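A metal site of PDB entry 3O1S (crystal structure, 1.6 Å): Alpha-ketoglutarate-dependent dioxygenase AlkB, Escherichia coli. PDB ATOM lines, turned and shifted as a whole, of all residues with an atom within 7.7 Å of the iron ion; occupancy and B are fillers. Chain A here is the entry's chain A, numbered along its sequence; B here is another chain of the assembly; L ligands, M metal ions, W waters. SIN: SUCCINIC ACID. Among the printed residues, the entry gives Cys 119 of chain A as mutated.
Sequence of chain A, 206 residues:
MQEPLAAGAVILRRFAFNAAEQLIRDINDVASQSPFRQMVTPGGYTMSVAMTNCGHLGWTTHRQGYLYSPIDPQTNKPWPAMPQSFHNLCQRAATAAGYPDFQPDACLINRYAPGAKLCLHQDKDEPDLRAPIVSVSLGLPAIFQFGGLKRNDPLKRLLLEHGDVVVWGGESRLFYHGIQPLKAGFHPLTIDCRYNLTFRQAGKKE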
ATOM      1  N   LEU A 108     -13.254 -20.511   8.456  1.00  0.00           N
ATOM      2  CA  LEU A 108     -12.633 -21.835   8.393  1.00  0.00           C
ATOM      3  C   LEU A 108     -12.928 -22.553   9.693  1.00  0.00           C
ATOM      4  O   LEU A 108     -12.703 -22.005  10.777  1.00  0.00           O
ATOM      5  CB  LEU A 108     -11.125 -21.676   8.200  1.00  0.00           C
ATOM      6  CG  LEU A 108     -10.260 -22.936   8.267  1.00  0.00           C
ATOM      7  CD1 LEU A 108     -10.594 -23.847   7.146  1.00  0.00           C
ATOM      8  CD2 LEU A 108      -8.787 -22.506   8.153  1.00  0.00           C
ATOM      9  N   ASN A 110     -12.026 -25.671  11.980  1.00  0.00           N
ATOM     10  CA  ASN A 110     -11.027 -26.708  12.244  1.00  0.00           C
ATOM     11  C   ASN A 110     -11.565 -27.680  13.293  1.00  0.00           C
ATOM     12  O   ASN A 110     -12.190 -27.261  14.280  1.00  0.00           O
ATOM     13  CB  ASN A 110      -9.705 -26.106  12.756  1.00  0.00           C
ATOM     14  CG  ASN A 110      -8.976 -25.238  11.726  1.00  0.00           C
ATOM     15  OD1 ASN A 110      -8.163 -24.416  12.103  1.00  0.00           O
ATOM     16  ND2 ASN A 110      -9.230 -25.436  10.444  1.00  0.00           N
ATOM     17  N   LEU A 118      -1.266 -27.782  14.590  1.00  0.00           N
ATOM     18  CA  LEU A 118      -1.002 -26.868  13.482  1.00  0.00           C
ATOM     19  C   LEU A 118       0.350 -26.254  13.718  1.00  0.00           C
ATOM     20  O   LEU A 118       0.518 -25.482  14.674  1.00  0.00           O
ATOM     21  CB  LEU A 118      -2.069 -25.773  13.430  1.00  0.00           C
ATOM     22  CG  LEU A 118      -2.670 -25.370  12.091  1.00  0.00           C
ATOM     23  CD1 LEU A 118      -3.079 -26.583  11.265  1.00  0.00           C
ATOM     24  CD2 LEU A 118      -3.876 -24.467  12.368  1.00  0.00           C
ATOM     25  N   CYS A 119       1.309 -26.599  12.882  1.00  0.00           N
ATOM     26  CA  CYS A 119       2.658 -26.060  13.021  1.00  0.00           C
ATOM     27  C   CYS A 119       2.646 -24.549  12.823  1.00  0.00           C
ATOM     28  O   CYS A 119       1.805 -24.033  12.096  1.00  0.00           O
ATOM     29  CB  CYS A 119       3.594 -26.727  12.020  1.00  0.00           C
ATOM     30  SG  CYS A 119       3.908 -28.457  12.473  1.00  0.00           S
ATOM     31  N   LEU A 120       3.583 -23.868  13.494  1.00  0.00           N
ATOM     32  CA  LEU A 120       3.708 -22.398  13.463  1.00  0.00           C
ATOM     33  C   LEU A 120       3.661 -21.870  12.037  1.00  0.00           C
ATOM     34  O   LEU A 120       4.441 -22.285  11.165  1.00  0.00           O
ATOM     35  CB  LEU A 120       5.015 -21.988  14.142  1.00  0.00           C
ATOM     36  CG  LEU A 120       5.084 -20.627  14.856  1.00  0.00           C
ATOM     37  CD1 LEU A 120       4.233 -20.686  16.132  1.00  0.00           C
ATOM     38  CD2 LEU A 120       6.523 -20.259  15.175  1.00  0.00           C
ATOM     39  N   HIS A 121       2.737 -20.941  11.779  1.00  0.00           N
ATOM     40  CA  HIS A 121       2.568 -20.378  10.450  1.00  0.00           C
ATOM     41  C   HIS A 121       2.099 -18.944  10.554  1.00  0.00           C
ATOM     42  O   HIS A 121       1.878 -18.434  11.645  1.00  0.00           O
ATOM     43  CB  HIS A 121       1.520 -21.165   9.649  1.00  0.00           C
ATOM     44  CG  HIS A 121       0.160 -21.161  10.258  1.00  0.00           C
ATOM     45  ND1 HIS A 121      -0.208 -22.032  11.251  1.00  0.00           N
ATOM     46  CD2 HIS A 121      -0.941 -20.402  10.005  1.00  0.00           C
ATOM     47  CE1 HIS A 121      -1.458 -21.816  11.598  1.00  0.00           C
ATOM     48  NE2 HIS A 121      -1.931 -20.825  10.853  1.00  0.00           N
ATOM     49  N   GLN A 122       1.960 -18.298   9.397  1.00  0.00           N
ATOM     50  CA  GLN A 122       1.394 -16.952   9.305  1.00  0.00           C
ATOM     51  C   GLN A 122       0.081 -16.997   8.528  1.00  0.00           C
ATOM     52  O   GLN A 122      -0.067 -17.808   7.602  1.00  0.00           O
ATOM     53  CB  GLN A 122       2.373 -15.998   8.622  1.00  0.00           C
ATOM     54  CG  GLN A 122       3.653 -15.755   9.390  1.00  0.00           C
ATOM     55  CD  GLN A 122       4.616 -14.872   8.615  1.00  0.00           C
ATOM     56  OE1 GLN A 122       5.095 -15.245   7.543  1.00  0.00           O
ATOM     57  NE2 GLN A 122       4.918 -13.693   9.161  1.00  0.00           N
ATOM     58  N   ASP A 123      -0.877 -16.156   8.899  1.00  0.00           N
ATOM     59  CA  ASP A 123      -2.068 -15.976   8.077  1.00  0.00           C
ATOM     60  C   ASP A 123      -1.785 -14.846   7.088  1.00  0.00           C
ATOM     61  O   ASP A 123      -1.724 -13.687   7.472  1.00  0.00           O
ATOM     62  CB  ASP A 123      -3.286 -15.642   8.938  1.00  0.00           C
ATOM     63  CG  ASP A 123      -3.939 -16.871   9.527  1.00  0.00           C
ATOM     64  OD1 ASP A 123      -3.238 -17.862   9.825  1.00  0.00           O
ATOM     65  OD2 ASP A 123      -5.175 -16.842   9.711  1.00  0.00           O
ATOM     66  N   LYS A 124      -1.608 -15.190   5.818  1.00  0.00           N
ATOM     67  CA  LYS A 124      -1.260 -14.185   4.821  1.00  0.00           C
ATOM     68  C   LYS A 124      -1.851 -14.429   3.441  1.00  0.00           C
ATOM     69  O   LYS A 124      -1.399 -13.853   2.440  1.00  0.00           O
ATOM     70  CB  LYS A 124       0.263 -14.041   4.725  1.00  0.00           C
ATOM     71  CG  LYS A 124       0.974 -15.313   4.306  1.00  0.00           C
ATOM     72  CD  LYS A 124       2.468 -15.087   4.175  1.00  0.00           C
ATOM     73  CE  LYS A 124       3.227 -16.391   4.042  1.00  0.00           C
ATOM     74  NZ  LYS A 124       4.701 -16.152   3.895  1.00  0.00           N
ATOM     75  N   GLU A 126      -4.811 -13.584   2.716  1.00  0.00           N
ATOM     76  CA  GLU A 126      -5.782 -12.502   2.530  1.00  0.00           C
ATOM     77  C   GLU A 126      -5.090 -11.249   1.963  1.00  0.00           C
ATOM     78  O   GLU A 126      -4.033 -10.838   2.447  1.00  0.00           O
ATOM     79  CB  GLU A 126      -6.473 -12.178   3.860  1.00  0.00           C
ATOM     80  CG  GLU A 126      -6.994 -13.379   4.628  1.00  0.00           C
ATOM     81  CD  GLU A 126      -5.879 -14.197   5.280  1.00  0.00           C
ATOM     82  OE1 GLU A 126      -4.900 -13.594   5.765  1.00  0.00           O
ATOM     83  OE2 GLU A 126      -5.996 -15.442   5.310  1.00  0.00           O
ATOM     84  N   ILE A 133      -8.026 -11.049  12.387  1.00  0.00           N
ATOM     85  CA  ILE A 133      -8.451 -12.436  12.446  1.00  0.00           C
ATOM     86  C   ILE A 133      -9.189 -12.643  13.763  1.00  0.00           C
ATOM     87  O   ILE A 133      -8.703 -12.254  14.818  1.00  0.00           O
ATOM     88  CB  ILE A 133      -7.242 -13.400  12.438  1.00  0.00           C
ATOM     89  CG1 ILE A 133      -6.302 -13.123  11.259  1.00  0.00           C
ATOM     90  CG2 ILE A 133      -7.744 -14.850  12.478  1.00  0.00           C
ATOM     91  CD1 ILE A 133      -6.841 -13.482   9.908  1.00  0.00           C
ATOM     92  N   SER A 135     -10.655 -15.680  16.161  1.00  0.00           N
ATOM     93  CA  SER A 135     -10.487 -17.117  16.337  1.00  0.00           C
ATOM     94  C   SER A 135     -11.252 -17.601  17.583  1.00  0.00           C
ATOM     95  O   SER A 135     -10.917 -17.189  18.696  1.00  0.00           O
ATOM     96  CB  SER A 135      -8.969 -17.400  16.470  1.00  0.00           C
ATOM     97  OG  SER A 135      -8.679 -18.787  16.454  1.00  0.00           O
ATOM     98  N   PHE A 144      -1.988 -22.695  22.495  1.00  0.00           N
ATOM     99  CA  PHE A 144      -1.849 -21.813  21.352  1.00  0.00           C
ATOM    100  C   PHE A 144      -0.500 -21.147  21.467  1.00  0.00           C
ATOM    101  O   PHE A 144      -0.133 -20.633  22.533  1.00  0.00           O
ATOM    102  CB  PHE A 144      -2.972 -20.762  21.426  1.00  0.00           C
ATOM    103  CG  PHE A 144      -2.963 -19.731  20.328  1.00  0.00           C
ATOM    104  CD1 PHE A 144      -3.171 -20.098  19.000  1.00  0.00           C
ATOM    105  CD2 PHE A 144      -2.860 -18.387  20.647  1.00  0.00           C
ATOM    106  CE1 PHE A 144      -3.251 -19.142  18.005  1.00  0.00           C
ATOM    107  CE2 PHE A 144      -2.920 -17.405  19.648  1.00  0.00           C
ATOM    108  CZ  PHE A 144      -3.096 -17.788  18.330  1.00  0.00           C
ATOM    109  N   TRP A 168      -6.488 -11.034  16.574  1.00  0.00           N
ATOM    110  CA  TRP A 168      -5.258 -10.329  16.277  1.00  0.00           C
ATOM    111  C   TRP A 168      -5.379  -9.543  14.984  1.00  0.00           C
ATOM    112  O   TRP A 168      -6.162  -9.878  14.085  1.00  0.00           O
ATOM    113  CB  TRP A 168      -4.006 -11.228  16.349  1.00  0.00           C
ATOM    114  CG  TRP A 168      -3.906 -12.375  15.379  1.00  0.00           C
ATOM    115  CD1 TRP A 168      -3.173 -12.415  14.223  1.00  0.00           C
ATOM    116  CD2 TRP A 168      -4.507 -13.674  15.517  1.00  0.00           C
ATOM    117  NE1 TRP A 168      -3.286 -13.640  13.629  1.00  0.00           N
ATOM    118  CE2 TRP A 168      -4.107 -14.437  14.398  1.00  0.00           C
ATOM    119  CE3 TRP A 168      -5.338 -14.259  16.465  1.00  0.00           C
ATOM    120  CZ2 TRP A 168      -4.513 -15.749  14.197  1.00  0.00           C
ATOM    121  CZ3 TRP A 168      -5.751 -15.577  16.268  1.00  0.00           C
ATOM    122  CH2 TRP A 168      -5.347 -16.298  15.140  1.00  0.00           C
ATOM    123  N   PHE A 175       1.723 -12.181  12.701  1.00  0.00           N
ATOM    124  CA  PHE A 175       2.555 -12.896  13.661  1.00  0.00           C
ATOM    125  C   PHE A 175       2.398 -14.390  13.453  1.00  0.00           C
ATOM    126  O   PHE A 175       1.322 -14.845  13.088  1.00  0.00           O
ATOM    127  CB  PHE A 175       2.187 -12.513  15.105  1.00  0.00           C
ATOM    128  CG  PHE A 175       2.767 -11.192  15.570  1.00  0.00           C
ATOM    129  CD1 PHE A 175       2.654 -10.800  16.891  1.00  0.00           C
ATOM    130  CD2 PHE A 175       3.458 -10.372  14.691  1.00  0.00           C
ATOM    131  CE1 PHE A 175       3.179  -9.598  17.325  1.00  0.00           C
ATOM    132  CE2 PHE A 175       4.007  -9.165  15.124  1.00  0.00           C
ATOM    133  CZ  PHE A 175       3.862  -8.783  16.450  1.00  0.00           C
ATOM    134  N   TYR A 176       3.471 -15.139  13.673  1.00  0.00           N
ATOM    135  CA  TYR A 176       3.423 -16.594  13.619  1.00  0.00           C
ATOM    136  C   TYR A 176       2.601 -17.105  14.785  1.00  0.00           C
ATOM    137  O   TYR A 176       2.709 -16.544  15.900  1.00  0.00           O
ATOM    138  CB  TYR A 176       4.846 -17.135  13.733  1.00  0.00           C
ATOM    139  CG  TYR A 176       5.602 -17.175  12.431  1.00  0.00           C
ATOM    140  CD1 TYR A 176       5.555 -18.299  11.617  1.00  0.00           C
ATOM    141  CD2 TYR A 176       6.358 -16.095  12.023  1.00  0.00           C
ATOM    142  CE1 TYR A 176       6.240 -18.355  10.431  1.00  0.00           C
ATOM    143  CE2 TYR A 176       7.048 -16.134  10.821  1.00  0.00           C
ATOM    144  CZ  TYR A 176       6.990 -17.257  10.034  1.00  0.00           C
ATOM    145  OH  TYR A 176       7.688 -17.292   8.850  1.00  0.00           O
ATOM    146  N   HIS A 177       1.831 -18.164  14.566  1.00  0.00           N
ATOM    147  CA  HIS A 177       1.029 -18.790  15.598  1.00  0.00           C
ATOM    148  C   HIS A 177       0.800 -20.234  15.201  1.00  0.00           C
ATOM    149  O   HIS A 177       1.024 -20.622  14.041  1.00  0.00           O
ATOM    150  CB  HIS A 177      -0.323 -18.062  15.719  1.00  0.00           C
ATOM    151  CG  HIS A 177      -1.056 -17.964  14.421  1.00  0.00           C
ATOM    152  ND1 HIS A 177      -0.725 -17.047  13.449  1.00  0.00           N
ATOM    153  CD2 HIS A 177      -2.057 -18.711  13.906  1.00  0.00           C
ATOM    154  CE1 HIS A 177      -1.522 -17.212  12.400  1.00  0.00           C
ATOM    155  NE2 HIS A 177      -2.338 -18.212  12.654  1.00  0.00           N
ATOM    156  N   GLY A 178       0.310 -21.024  16.147  1.00  0.00           N
ATOM    157  CA  GLY A 178       0.102 -22.442  15.927  1.00  0.00           C
ATOM    158  C   GLY A 178      -0.576 -23.077  17.104  1.00  0.00           C
ATOM    159  O   GLY A 178      -0.870 -22.397  18.109  1.00  0.00           O
ATOM    160  N   ASN A 196     -12.297 -25.085  16.221  1.00  0.00           N
ATOM    161  CA  ASN A 196     -11.946 -23.675  16.160  1.00  0.00           C
ATOM    162  C   ASN A 196     -12.621 -23.023  14.945  1.00  0.00           C
ATOM    163  O   ASN A 196     -12.663 -23.616  13.850  1.00  0.00           O
ATOM    164  CB  ASN A 196     -10.438 -23.541  16.051  1.00  0.00           C
ATOM    165  CG  ASN A 196      -9.984 -22.101  15.856  1.00  0.00           C
ATOM    166  OD1 ASN A 196      -9.776 -21.651  14.738  1.00  0.00           O
ATOM    167  ND2 ASN A 196      -9.829 -21.395  16.955  1.00  0.00           N
ATOM    168  N   THR A 198     -12.259 -19.770  12.565  1.00  0.00           N
ATOM    169  CA  THR A 198     -11.400 -18.666  12.215  1.00  0.00           C
ATOM    170  C   THR A 198     -12.057 -17.794  11.165  1.00  0.00           C
ATOM    171  O   THR A 198     -12.245 -18.222  10.018  1.00  0.00           O
ATOM    172  CB  THR A 198     -10.048 -19.156  11.713  1.00  0.00           C
ATOM    173  OG1 THR A 198      -9.389 -19.858  12.776  1.00  0.00           O
ATOM    174  CG2 THR A 198      -9.227 -17.942  11.350  1.00  0.00           C
ATOM    175  N   ARG A 200     -12.170 -14.488   8.700  1.00  0.00           N
ATOM    176  CA  ARG A 200     -11.301 -13.558   7.995  1.00  0.00           C
ATOM    177  C   ARG A 200     -12.077 -12.781   6.951  1.00  0.00           C
ATOM    178  O   ARG A 200     -13.145 -13.184   6.528  1.00  0.00           O
ATOM    179  CB  ARG A 200     -10.159 -14.312   7.305  1.00  0.00           C
ATOM    180  CG  ARG A 200      -9.248 -15.078   8.236  1.00  0.00           C
ATOM    181  CD  ARG A 200      -8.253 -15.887   7.402  1.00  0.00           C
ATOM    182  NE  ARG A 200      -7.470 -16.830   8.181  1.00  0.00           N
ATOM    183  CZ  ARG A 200      -7.824 -18.086   8.428  1.00  0.00           C
ATOM    184  NH1 ARG A 200      -8.977 -18.555   7.967  1.00  0.00           N
ATOM    185  NH2 ARG A 200      -7.039 -18.883   9.144  1.00  0.00           N
ATOM    186  P   MDQ B   7       3.271 -23.301   6.437  1.00  0.00           P
ATOM    187  N1  MDQ B   7      -1.501 -23.581   7.514  1.00  0.00           N
ATOM    188  C2  MDQ B   7      -2.836 -23.242   7.789  1.00  0.00           C
ATOM    189  O2  MDQ B   7      -3.561 -24.027   8.432  1.00  0.00           O
ATOM    190  N3  MDQ B   7      -3.339 -22.081   7.342  1.00  0.00           N
ATOM    191  C4  MDQ B   7      -2.546 -21.229   6.643  1.00  0.00           C
ATOM    192  N4  MDQ B   7      -3.078 -20.025   6.180  1.00  0.00           N
ATOM    193  C5  MDQ B   7      -1.225 -21.555   6.384  1.00  0.00           C
ATOM    194  C6  MDQ B   7      -0.691 -22.745   6.845  1.00  0.00           C
ATOM    195  C1' MDQ B   7      -0.956 -24.834   8.049  1.00  0.00           C
ATOM    196  O1P MDQ B   7       3.581 -22.244   7.452  1.00  0.00           O
ATOM    197  C2' MDQ B   7      -0.353 -25.774   7.012  1.00  0.00           C
ATOM    198  C20 MDQ B   7      -4.820 -22.105   7.226  1.00  0.00           C
ATOM    199  O21 MDQ B   7      -5.645 -21.234   7.258  1.00  0.00           O
ATOM    200  O2P MDQ B   7       2.603 -22.879   5.149  1.00  0.00           O
ATOM    201  C3' MDQ B   7       0.635 -26.551   7.874  1.00  0.00           C
ATOM    202  O3' MDQ B   7      -0.158 -27.547   8.554  1.00  0.00           O
ATOM    203  C4' MDQ B   7       1.117 -25.493   8.851  1.00  0.00           C
ATOM    204  O4' MDQ B   7       0.141 -24.443   8.866  1.00  0.00           O
ATOM    205  C5' MDQ B   7       2.435 -24.867   8.415  1.00  0.00           C
ATOM    206  O5' MDQ B   7       2.311 -24.440   7.056  1.00  0.00           O
HETATM  207  C1  SIN L   1      -5.402 -21.414  12.813  1.00  0.00           C
HETATM  208  O1  SIN L   1      -5.718 -21.529  11.603  1.00  0.00           O
HETATM  209  O2  SIN L   1      -4.367 -20.797  13.134  1.00  0.00           O
HETATM  210  C2  SIN L   1      -6.284 -22.035  13.860  1.00  0.00           C
HETATM  211  C3  SIN L   1      -5.734 -21.771  15.246  1.00  0.00           C
HETATM  212  C4  SIN L   1      -6.623 -22.533  16.221  1.00  0.00           C
HETATM  213  O3  SIN L   1      -7.083 -23.663  15.933  1.00  0.00           O
HETATM  214  O4  SIN L   1      -6.907 -22.033  17.333  1.00  0.00           O
HETATM  215 FE    FE M   1      -3.569 -19.397  11.363  1.00  0.00          FE
HETATM  216  O   HOH W   1      -5.485 -18.258  11.881  1.00  0.00           O
HETATM  217  O   HOH W   2      -4.560 -20.337   9.855  1.00  0.00           O
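ND1 of His 177 lies within hydrogen-bond range of O of Phe 175, 3.0 Å away. The side-chain carboxylate (OD2) of Asp 123 lies within salt-bridge range of the guanidinium group (NE) of Arg 200 (2.8 Å). O4' of MDQ 7 of chain B sits at hydrogen-bond distance from ND1 of His 121, at 3.4 Å. The backbone carbonyl oxygen (O) of Cys 119 is in hydrogen-bond range of a ring nitrogen (ND1) of His 121 (3.0 Å).
The nearest printed residue that does not touch the iron ion is Arg 200 (4.2 Å).
The iron ion is bound by water W2, NE2 of His 177, OD1 of Asp 123, NE2 of His 121, water W1 and O2 of the ligand.
Water W2 lies within hydrogen-bond range of O21 of MDQ 7 of chain B (3.0 Å) and NH2 of Arg 200 (3.0 Å). Water W1 bridges the side-chain carboxylate of Asp 123 (2.6 Å) and the guanidinium group of Arg 200 (3.2 Å).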
